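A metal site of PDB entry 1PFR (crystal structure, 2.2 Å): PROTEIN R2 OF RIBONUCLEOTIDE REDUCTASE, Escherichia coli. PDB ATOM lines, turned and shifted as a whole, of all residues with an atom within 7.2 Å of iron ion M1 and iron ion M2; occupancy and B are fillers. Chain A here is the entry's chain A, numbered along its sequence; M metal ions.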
ATOM      1  N   GLN A  80      -8.246   7.973 -11.511  1.00  0.00           N
ATOM      2  CA  GLN A  80      -8.462   7.181 -12.700  1.00  0.00           C
ATOM      3  C   GLN A  80      -7.218   6.344 -12.937  1.00  0.00           C
ATOM      4  O   GLN A  80      -7.324   5.210 -13.351  1.00  0.00           O
ATOM      5  CB  GLN A  80      -8.753   8.045 -13.924  1.00  0.00           C
ATOM      6  CG  GLN A  80      -9.972   8.947 -13.801  1.00  0.00           C
ATOM      7  CD  GLN A  80     -10.008   9.972 -14.913  1.00  0.00           C
ATOM      8  OE1 GLN A  80      -9.286  10.966 -14.899  1.00  0.00           O
ATOM      9  NE2 GLN A  80     -10.811   9.696 -15.920  1.00  0.00           N
ATOM     10  N   LEU A  83      -7.436   3.149 -10.922  1.00  0.00           N
ATOM     11  CA  LEU A  83      -8.384   2.190 -11.447  1.00  0.00           C
ATOM     12  C   LEU A  83      -7.964   1.478 -12.697  1.00  0.00           C
ATOM     13  O   LEU A  83      -8.107   0.275 -12.823  1.00  0.00           O
ATOM     14  CB  LEU A  83      -9.775   2.798 -11.686  1.00  0.00           C
ATOM     15  CG  LEU A  83     -10.586   3.439 -10.550  1.00  0.00           C
ATOM     16  CD1 LEU A  83     -11.851   4.118 -11.095  1.00  0.00           C
ATOM     17  CD2 LEU A  83     -10.866   2.609  -9.292  1.00  0.00           C
ATOM     18  N   ASP A  84      -7.545   2.254 -13.682  1.00  0.00           N
ATOM     19  CA  ASP A  84      -7.148   1.679 -14.950  1.00  0.00           C
ATOM     20  C   ASP A  84      -5.909   0.822 -14.793  1.00  0.00           C
ATOM     21  O   ASP A  84      -5.748  -0.130 -15.554  1.00  0.00           O
ATOM     22  CB  ASP A  84      -7.012   2.733 -16.031  1.00  0.00           C
ATOM     23  CG  ASP A  84      -8.354   3.026 -16.679  1.00  0.00           C
ATOM     24  OD1 ASP A  84      -9.224   2.127 -16.638  1.00  0.00           O
ATOM     25  OD2 ASP A  84      -8.611   4.131 -17.181  1.00  0.00           O
ATOM     26  N   SER A  85      -5.076   1.103 -13.789  1.00  0.00           N
ATOM     27  CA  SER A  85      -3.855   0.323 -13.539  1.00  0.00           C
ATOM     28  C   SER A  85      -4.365  -1.043 -13.121  1.00  0.00           C
ATOM     29  O   SER A  85      -3.926  -2.113 -13.572  1.00  0.00           O
ATOM     30  CB  SER A  85      -3.074   0.891 -12.329  1.00  0.00           C
ATOM     31  OG  SER A  85      -2.324   2.053 -12.662  1.00  0.00           O
ATOM     32  N   GLN A  87      -7.386  -2.226 -13.672  1.00  0.00           N
ATOM     33  CA  GLN A  87      -8.175  -2.814 -14.742  1.00  0.00           C
ATOM     34  C   GLN A  87      -7.390  -3.333 -15.920  1.00  0.00           C
ATOM     35  O   GLN A  87      -7.904  -4.139 -16.686  1.00  0.00           O
ATOM     36  CB  GLN A  87      -9.335  -1.936 -15.227  1.00  0.00           C
ATOM     37  CG  GLN A  87     -10.406  -1.848 -14.168  1.00  0.00           C
ATOM     38  CD  GLN A  87     -11.066  -3.183 -13.868  1.00  0.00           C
ATOM     39  OE1 GLN A  87     -10.693  -3.915 -12.957  1.00  0.00           O
ATOM     40  NE2 GLN A  87     -12.072  -3.486 -14.655  1.00  0.00           N
ATOM     41  N   GLY A  88      -6.147  -2.913 -16.028  1.00  0.00           N
ATOM     42  CA  GLY A  88      -5.334  -3.399 -17.124  1.00  0.00           C
ATOM     43  C   GLY A  88      -4.849  -4.829 -16.934  1.00  0.00           C
ATOM     44  O   GLY A  88      -4.866  -5.594 -17.885  1.00  0.00           O
ATOM     45  N   TRP A 111     -10.654  -6.297 -23.793  1.00  0.00           N
ATOM     46  CA  TRP A 111     -11.088  -5.365 -22.738  1.00  0.00           C
ATOM     47  C   TRP A 111      -9.950  -4.926 -21.829  1.00  0.00           C
ATOM     48  O   TRP A 111      -9.878  -3.763 -21.471  1.00  0.00           O
ATOM     49  CB  TRP A 111     -12.201  -6.047 -21.923  1.00  0.00           C
ATOM     50  CG  TRP A 111     -12.527  -5.490 -20.557  1.00  0.00           C
ATOM     51  CD1 TRP A 111     -12.275  -4.223 -20.049  1.00  0.00           C
ATOM     52  CD2 TRP A 111     -13.199  -6.205 -19.527  1.00  0.00           C
ATOM     53  NE1 TRP A 111     -12.799  -4.120 -18.770  1.00  0.00           N
ATOM     54  CE2 TRP A 111     -13.339  -5.331 -18.410  1.00  0.00           C
ATOM     55  CE3 TRP A 111     -13.693  -7.518 -19.424  1.00  0.00           C
ATOM     56  CZ2 TRP A 111     -13.951  -5.725 -17.228  1.00  0.00           C
ATOM     57  CZ3 TRP A 111     -14.315  -7.900 -18.255  1.00  0.00           C
ATOM     58  CH2 TRP A 111     -14.418  -7.022 -17.161  1.00  0.00           C
ATOM     59  N   SER A 114      -7.638  -2.513 -23.857  1.00  0.00           N
ATOM     60  CA  SER A 114      -8.149  -1.144 -23.990  1.00  0.00           C
ATOM     61  C   SER A 114      -7.946  -0.354 -22.673  1.00  0.00           C
ATOM     62  O   SER A 114      -7.747   0.863 -22.697  1.00  0.00           O
ATOM     63  CB  SER A 114      -9.608  -1.225 -24.460  1.00  0.00           C
ATOM     64  OG  SER A 114     -10.464  -1.526 -23.364  1.00  0.00           O
ATOM     65  N   GLU A 115      -7.897  -1.040 -21.525  1.00  0.00           N
ATOM     66  CA  GLU A 115      -7.656  -0.338 -20.264  1.00  0.00           C
ATOM     67  C   GLU A 115      -6.236   0.171 -20.248  1.00  0.00           C
ATOM     68  O   GLU A 115      -5.962   1.225 -19.681  1.00  0.00           O
ATOM     69  CB  GLU A 115      -7.928  -1.192 -19.033  1.00  0.00           C
ATOM     70  CG  GLU A 115      -9.318  -1.866 -19.000  1.00  0.00           C
ATOM     71  CD  GLU A 115     -10.475  -0.905 -18.663  1.00  0.00           C
ATOM     72  OE1 GLU A 115     -10.567   0.221 -19.179  1.00  0.00           O
ATOM     73  OE2 GLU A 115     -11.381  -1.277 -17.906  1.00  0.00           O
ATOM     74  N   THR A 116      -5.334  -0.531 -20.915  1.00  0.00           N
ATOM     75  CA  THR A 116      -3.918  -0.096 -20.943  1.00  0.00           C
ATOM     76  C   THR A 116      -3.752   1.116 -21.807  1.00  0.00           C
ATOM     77  O   THR A 116      -2.884   1.946 -21.557  1.00  0.00           O
ATOM     78  CB  THR A 116      -2.917  -1.269 -21.298  1.00  0.00           C
ATOM     79  OG1 THR A 116      -3.024  -1.614 -22.673  1.00  0.00           O
ATOM     80  CG2 THR A 116      -3.331  -2.529 -20.471  1.00  0.00           C
ATOM     81  N   ILE A 117      -4.630   1.227 -22.806  1.00  0.00           N
ATOM     82  CA  ILE A 117      -4.640   2.402 -23.660  1.00  0.00           C
ATOM     83  C   ILE A 117      -5.034   3.551 -22.709  1.00  0.00           C
ATOM     84  O   ILE A 117      -4.338   4.566 -22.657  1.00  0.00           O
ATOM     85  CB  ILE A 117      -5.665   2.297 -24.778  1.00  0.00           C
ATOM     86  CG1 ILE A 117      -5.326   1.144 -25.707  1.00  0.00           C
ATOM     87  CG2 ILE A 117      -5.565   3.559 -25.595  1.00  0.00           C
ATOM     88  CD1 ILE A 117      -3.891   1.162 -26.117  1.00  0.00           C
ATOM     89  N   HIS A 118      -6.088   3.392 -21.902  1.00  0.00           N
ATOM     90  CA  HIS A 118      -6.451   4.438 -20.940  1.00  0.00           C
ATOM     91  C   HIS A 118      -5.310   4.872 -20.068  1.00  0.00           C
ATOM     92  O   HIS A 118      -5.117   6.056 -19.875  1.00  0.00           O
ATOM     93  CB  HIS A 118      -7.636   3.956 -20.098  1.00  0.00           C
ATOM     94  CG  HIS A 118      -8.826   3.681 -20.949  1.00  0.00           C
ATOM     95  ND1 HIS A 118      -9.970   3.041 -20.514  1.00  0.00           N
ATOM     96  CD2 HIS A 118      -9.007   3.877 -22.278  1.00  0.00           C
ATOM     97  CE1 HIS A 118     -10.804   2.877 -21.522  1.00  0.00           C
ATOM     98  NE2 HIS A 118     -10.240   3.367 -22.602  1.00  0.00           N
ATOM     99  N   SER A 119      -4.570   3.910 -19.536  1.00  0.00           N
ATOM    100  CA  SER A 119      -3.451   4.219 -18.663  1.00  0.00           C
ATOM    101  C   SER A 119      -2.435   5.108 -19.366  1.00  0.00           C
ATOM    102  O   SER A 119      -1.975   6.093 -18.815  1.00  0.00           O
ATOM    103  CB  SER A 119      -2.743   2.923 -18.269  1.00  0.00           C
ATOM    104  OG  SER A 119      -3.445   2.307 -17.193  1.00  0.00           O
ATOM    105  N   TYR A 122      -3.353   8.710 -19.566  1.00  0.00           N
ATOM    106  CA  TYR A 122      -3.091   9.530 -18.374  1.00  0.00           C
ATOM    107  C   TYR A 122      -1.671  10.074 -18.343  1.00  0.00           C
ATOM    108  O   TYR A 122      -1.424  11.209 -17.943  1.00  0.00           O
ATOM    109  CB  TYR A 122      -3.353   8.723 -17.109  1.00  0.00           C
ATOM    110  CG  TYR A 122      -4.770   8.240 -17.091  1.00  0.00           C
ATOM    111  CD1 TYR A 122      -5.810   9.019 -17.584  1.00  0.00           C
ATOM    112  CD2 TYR A 122      -5.071   6.953 -16.642  1.00  0.00           C
ATOM    113  CE1 TYR A 122      -7.142   8.544 -17.592  1.00  0.00           C
ATOM    114  CE2 TYR A 122      -6.398   6.463 -16.652  1.00  0.00           C
ATOM    115  CZ  TYR A 122      -7.422   7.262 -17.125  1.00  0.00           C
ATOM    116  OH  TYR A 122      -8.726   6.778 -17.131  1.00  0.00           O
ATOM    117  N   VAL A 200     -16.725  -5.786 -10.354  1.00  0.00           N
ATOM    118  CA  VAL A 200     -16.151  -5.146 -11.540  1.00  0.00           C
ATOM    119  C   VAL A 200     -17.222  -4.291 -12.217  1.00  0.00           C
ATOM    120  O   VAL A 200     -17.012  -3.205 -12.754  1.00  0.00           O
ATOM    121  CB  VAL A 200     -15.684  -6.202 -12.559  1.00  0.00           C
ATOM    122  CG1 VAL A 200     -15.251  -5.521 -13.831  1.00  0.00           C
ATOM    123  CG2 VAL A 200     -14.519  -7.011 -11.928  1.00  0.00           C
ATOM    124  N   LEU A 203     -17.655  -1.104 -10.492  1.00  0.00           N
ATOM    125  CA  LEU A 203     -16.517  -0.286 -10.862  1.00  0.00           C
ATOM    126  C   LEU A 203     -16.821   0.353 -12.207  1.00  0.00           C
ATOM    127  O   LEU A 203     -16.780   1.576 -12.334  1.00  0.00           O
ATOM    128  CB  LEU A 203     -15.275  -1.161 -10.919  1.00  0.00           C
ATOM    129  CG  LEU A 203     -13.925  -0.757 -11.513  1.00  0.00           C
ATOM    130  CD1 LEU A 203     -13.858   0.662 -11.901  1.00  0.00           C
ATOM    131  CD2 LEU A 203     -12.767  -1.079 -10.600  1.00  0.00           C
ATOM    132  N   GLU A 204     -17.156  -0.482 -13.206  1.00  0.00           N
ATOM    133  CA  GLU A 204     -17.482  -0.016 -14.560  1.00  0.00           C
ATOM    134  C   GLU A 204     -18.738   0.851 -14.666  1.00  0.00           C
ATOM    135  O   GLU A 204     -18.776   1.749 -15.508  1.00  0.00           O
ATOM    136  CB  GLU A 204     -17.692  -1.145 -15.572  1.00  0.00           C
ATOM    137  CG  GLU A 204     -16.526  -2.086 -15.868  1.00  0.00           C
ATOM    138  CD  GLU A 204     -15.389  -1.456 -16.655  1.00  0.00           C
ATOM    139  OE1 GLU A 204     -15.534  -0.300 -17.091  1.00  0.00           O
ATOM    140  OE2 GLU A 204     -14.363  -2.116 -16.850  1.00  0.00           O
ATOM    141  N   PHE A 208     -16.323   5.692 -12.419  1.00  0.00           N
ATOM    142  CA  PHE A 208     -15.716   6.703 -13.285  1.00  0.00           C
ATOM    143  C   PHE A 208     -16.486   8.029 -13.397  1.00  0.00           C
ATOM    144  O   PHE A 208     -15.931   9.123 -13.656  1.00  0.00           O
ATOM    145  CB  PHE A 208     -15.547   6.090 -14.672  1.00  0.00           C
ATOM    146  CG  PHE A 208     -14.358   5.169 -14.788  1.00  0.00           C
ATOM    147  CD1 PHE A 208     -13.051   5.682 -14.804  1.00  0.00           C
ATOM    148  CD2 PHE A 208     -14.561   3.776 -14.895  1.00  0.00           C
ATOM    149  CE1 PHE A 208     -11.963   4.840 -14.929  1.00  0.00           C
ATOM    150  CE2 PHE A 208     -13.483   2.896 -14.999  1.00  0.00           C
ATOM    151  CZ  PHE A 208     -12.170   3.428 -15.004  1.00  0.00           C
ATOM    152  N   ILE A 234     -12.439   7.549 -23.631  1.00  0.00           N
ATOM    153  CA  ILE A 234     -12.371   6.583 -22.582  1.00  0.00           C
ATOM    154  C   ILE A 234     -13.781   6.193 -22.188  1.00  0.00           C
ATOM    155  O   ILE A 234     -14.114   5.007 -22.099  1.00  0.00           O
ATOM    156  CB  ILE A 234     -11.675   7.192 -21.380  1.00  0.00           C
ATOM    157  CG1 ILE A 234     -10.155   7.148 -21.620  1.00  0.00           C
ATOM    158  CG2 ILE A 234     -12.110   6.460 -20.104  1.00  0.00           C
ATOM    159  CD1 ILE A 234      -9.320   7.676 -20.500  1.00  0.00           C
ATOM    160  N   ASP A 237     -15.385   3.775 -24.319  1.00  0.00           N
ATOM    161  CA  ASP A 237     -14.897   2.396 -24.132  1.00  0.00           C
ATOM    162  C   ASP A 237     -15.566   1.812 -22.857  1.00  0.00           C
ATOM    163  O   ASP A 237     -16.025   0.671 -22.816  1.00  0.00           O
ATOM    164  CB  ASP A 237     -13.366   2.373 -23.894  1.00  0.00           C
ATOM    165  CG  ASP A 237     -12.537   2.625 -25.148  1.00  0.00           C
ATOM    166  OD1 ASP A 237     -12.957   2.293 -26.293  1.00  0.00           O
ATOM    167  OD2 ASP A 237     -11.417   3.146 -24.972  1.00  0.00           O
ATOM    168  N   GLU A 238     -15.579   2.573 -21.764  1.00  0.00           N
ATOM    169  CA  GLU A 238     -16.170   2.039 -20.551  1.00  0.00           C
ATOM    170  C   GLU A 238     -17.633   1.615 -20.751  1.00  0.00           C
ATOM    171  O   GLU A 238     -18.109   0.665 -20.127  1.00  0.00           O
ATOM    172  CB  GLU A 238     -16.051   3.063 -19.426  1.00  0.00           C
ATOM    173  CG  GLU A 238     -14.607   3.602 -19.176  1.00  0.00           C
ATOM    174  CD  GLU A 238     -13.591   2.552 -18.698  1.00  0.00           C
ATOM    175  OE1 GLU A 238     -13.754   1.344 -18.980  1.00  0.00           O
ATOM    176  OE2 GLU A 238     -12.591   2.916 -18.066  1.00  0.00           O
ATOM    177  N   ALA A 239     -18.365   2.299 -21.630  1.00  0.00           N
ATOM    178  CA  ALA A 239     -19.760   1.897 -21.861  1.00  0.00           C
ATOM    179  C   ALA A 239     -19.822   0.486 -22.407  1.00  0.00           C
ATOM    180  O   ALA A 239     -20.707  -0.287 -22.052  1.00  0.00           O
ATOM    181  CB  ALA A 239     -20.471   2.880 -22.851  1.00  0.00           C
ATOM    182  N   LEU A 240     -18.886   0.142 -23.294  1.00  0.00           N
ATOM    183  CA  LEU A 240     -18.856  -1.203 -23.867  1.00  0.00           C
ATOM    184  C   LEU A 240     -18.488  -2.182 -22.754  1.00  0.00           C
ATOM    185  O   LEU A 240     -19.080  -3.235 -22.628  1.00  0.00           O
ATOM    186  CB  LEU A 240     -17.782  -1.299 -24.950  1.00  0.00           C
ATOM    187  CG  LEU A 240     -18.252  -1.225 -26.393  1.00  0.00           C
ATOM    188  CD1 LEU A 240     -17.049  -1.588 -27.284  1.00  0.00           C
ATOM    189  CD2 LEU A 240     -19.448  -2.157 -26.633  1.00  0.00           C
ATOM    190  N   HIS A 241     -17.488  -1.841 -21.945  1.00  0.00           N
ATOM    191  CA  HIS A 241     -17.090  -2.740 -20.877  1.00  0.00           C
ATOM    192  C   HIS A 241     -18.280  -3.089 -19.994  1.00  0.00           C
ATOM    193  O   HIS A 241     -18.551  -4.265 -19.700  1.00  0.00           O
ATOM    194  CB  HIS A 241     -15.994  -2.076 -20.064  1.00  0.00           C
ATOM    195  CG  HIS A 241     -14.790  -1.771 -20.919  1.00  0.00           C
ATOM    196  ND1 HIS A 241     -13.646  -1.151 -20.480  1.00  0.00           N
ATOM    197  CD2 HIS A 241     -14.609  -2.028 -22.238  1.00  0.00           C
ATOM    198  CE1 HIS A 241     -12.798  -1.008 -21.493  1.00  0.00           C
ATOM    199  NE2 HIS A 241     -13.365  -1.545 -22.565  1.00  0.00           N
ATOM    200  N   LEU A 242     -18.996  -2.047 -19.571  1.00  0.00           N
ATOM    201  CA  LEU A 242     -20.156  -2.234 -18.709  1.00  0.00           C
ATOM    202  C   LEU A 242     -21.203  -3.074 -19.437  1.00  0.00           C
ATOM    203  O   LEU A 242     -21.803  -3.974 -18.888  1.00  0.00           O
ATOM    204  CB  LEU A 242     -20.766  -0.862 -18.373  1.00  0.00           C
ATOM    205  CG  LEU A 242     -22.172  -0.893 -17.722  1.00  0.00           C
ATOM    206  CD1 LEU A 242     -22.427   0.345 -16.905  1.00  0.00           C
ATOM    207  CD2 LEU A 242     -23.123  -0.823 -18.883  1.00  0.00           C
HETATM  208 FE    FE M   1     -13.308  -0.353 -18.246  1.00  0.00          FE
HETATM  209 FE    FE M   2     -10.438   2.244 -18.347  1.00  0.00          FE
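A ring nitrogen (NE2) of His 118 lies within hydrogen-bond range of the side-chain carboxylate (OD2) of Asp 237 (2.7 Å).
OH of Tyr 122 is in hydrogen-bond range of OD2 of Asp 84 (2.6 Å).
The backbone carbonyl oxygen (O) of Trp 111 is in hydrogen-bond range of the side-chain hydroxyl (OG) of Ser 114 (3.0 Å).
NE2 of Gln 87 sits close to OE2 of Glu 204, 3.5 Å away.
A ring nitrogen (NE2) of His 241 sits close to the backbone carbonyl oxygen of Asp 237.
OE2 of Glu 204 sits close to NE1 of Trp 111.
A ring nitrogen (NE2) of His 241 lies within hydrogen-bond range of the side-chain hydroxyl (OG) of Ser 114 (3.0 Å).
The indole nitrogen (NE1) of Trp 111 sits close to the side-chain carboxylate (OE2) of Glu 115, 3.3 Å away.
Residues that only touch iron ion M1: Trp 111 (3.8 Å).
Within 4 Å of iron ion M1: Trp 111, Glu 115, Glu 204, Glu 238 and His 241.
Residues that only touch iron ion M2: Phe 208 (3.9 Å).
The nearest printed residue that does not touch iron ion M2 is Ile 234 (4.9 Å).
Iron ion M1 is bound by the side-chain carboxylate (OE1) of Glu 238 (1.9 Å), the side-chain carboxylate (OE2) of Glu 115 (2.2 Å), a ring nitrogen (ND1) of His 241 (2.4 Å), the side-chain carboxylate (OE2) of Glu 204 (2.5 Å) and the side-chain carboxylate (OE1) of Glu 204 (2.5 Å).
Iron ion M2 is bound by the side-chain carboxylate of Asp 84 (2.1 Å), the side-chain carboxylate of Glu 115 (2.2 Å), the side-chain carboxylate of Glu 238 (2.3 Å) and a ring nitrogen (ND1) of His 118 (2.4 Å).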
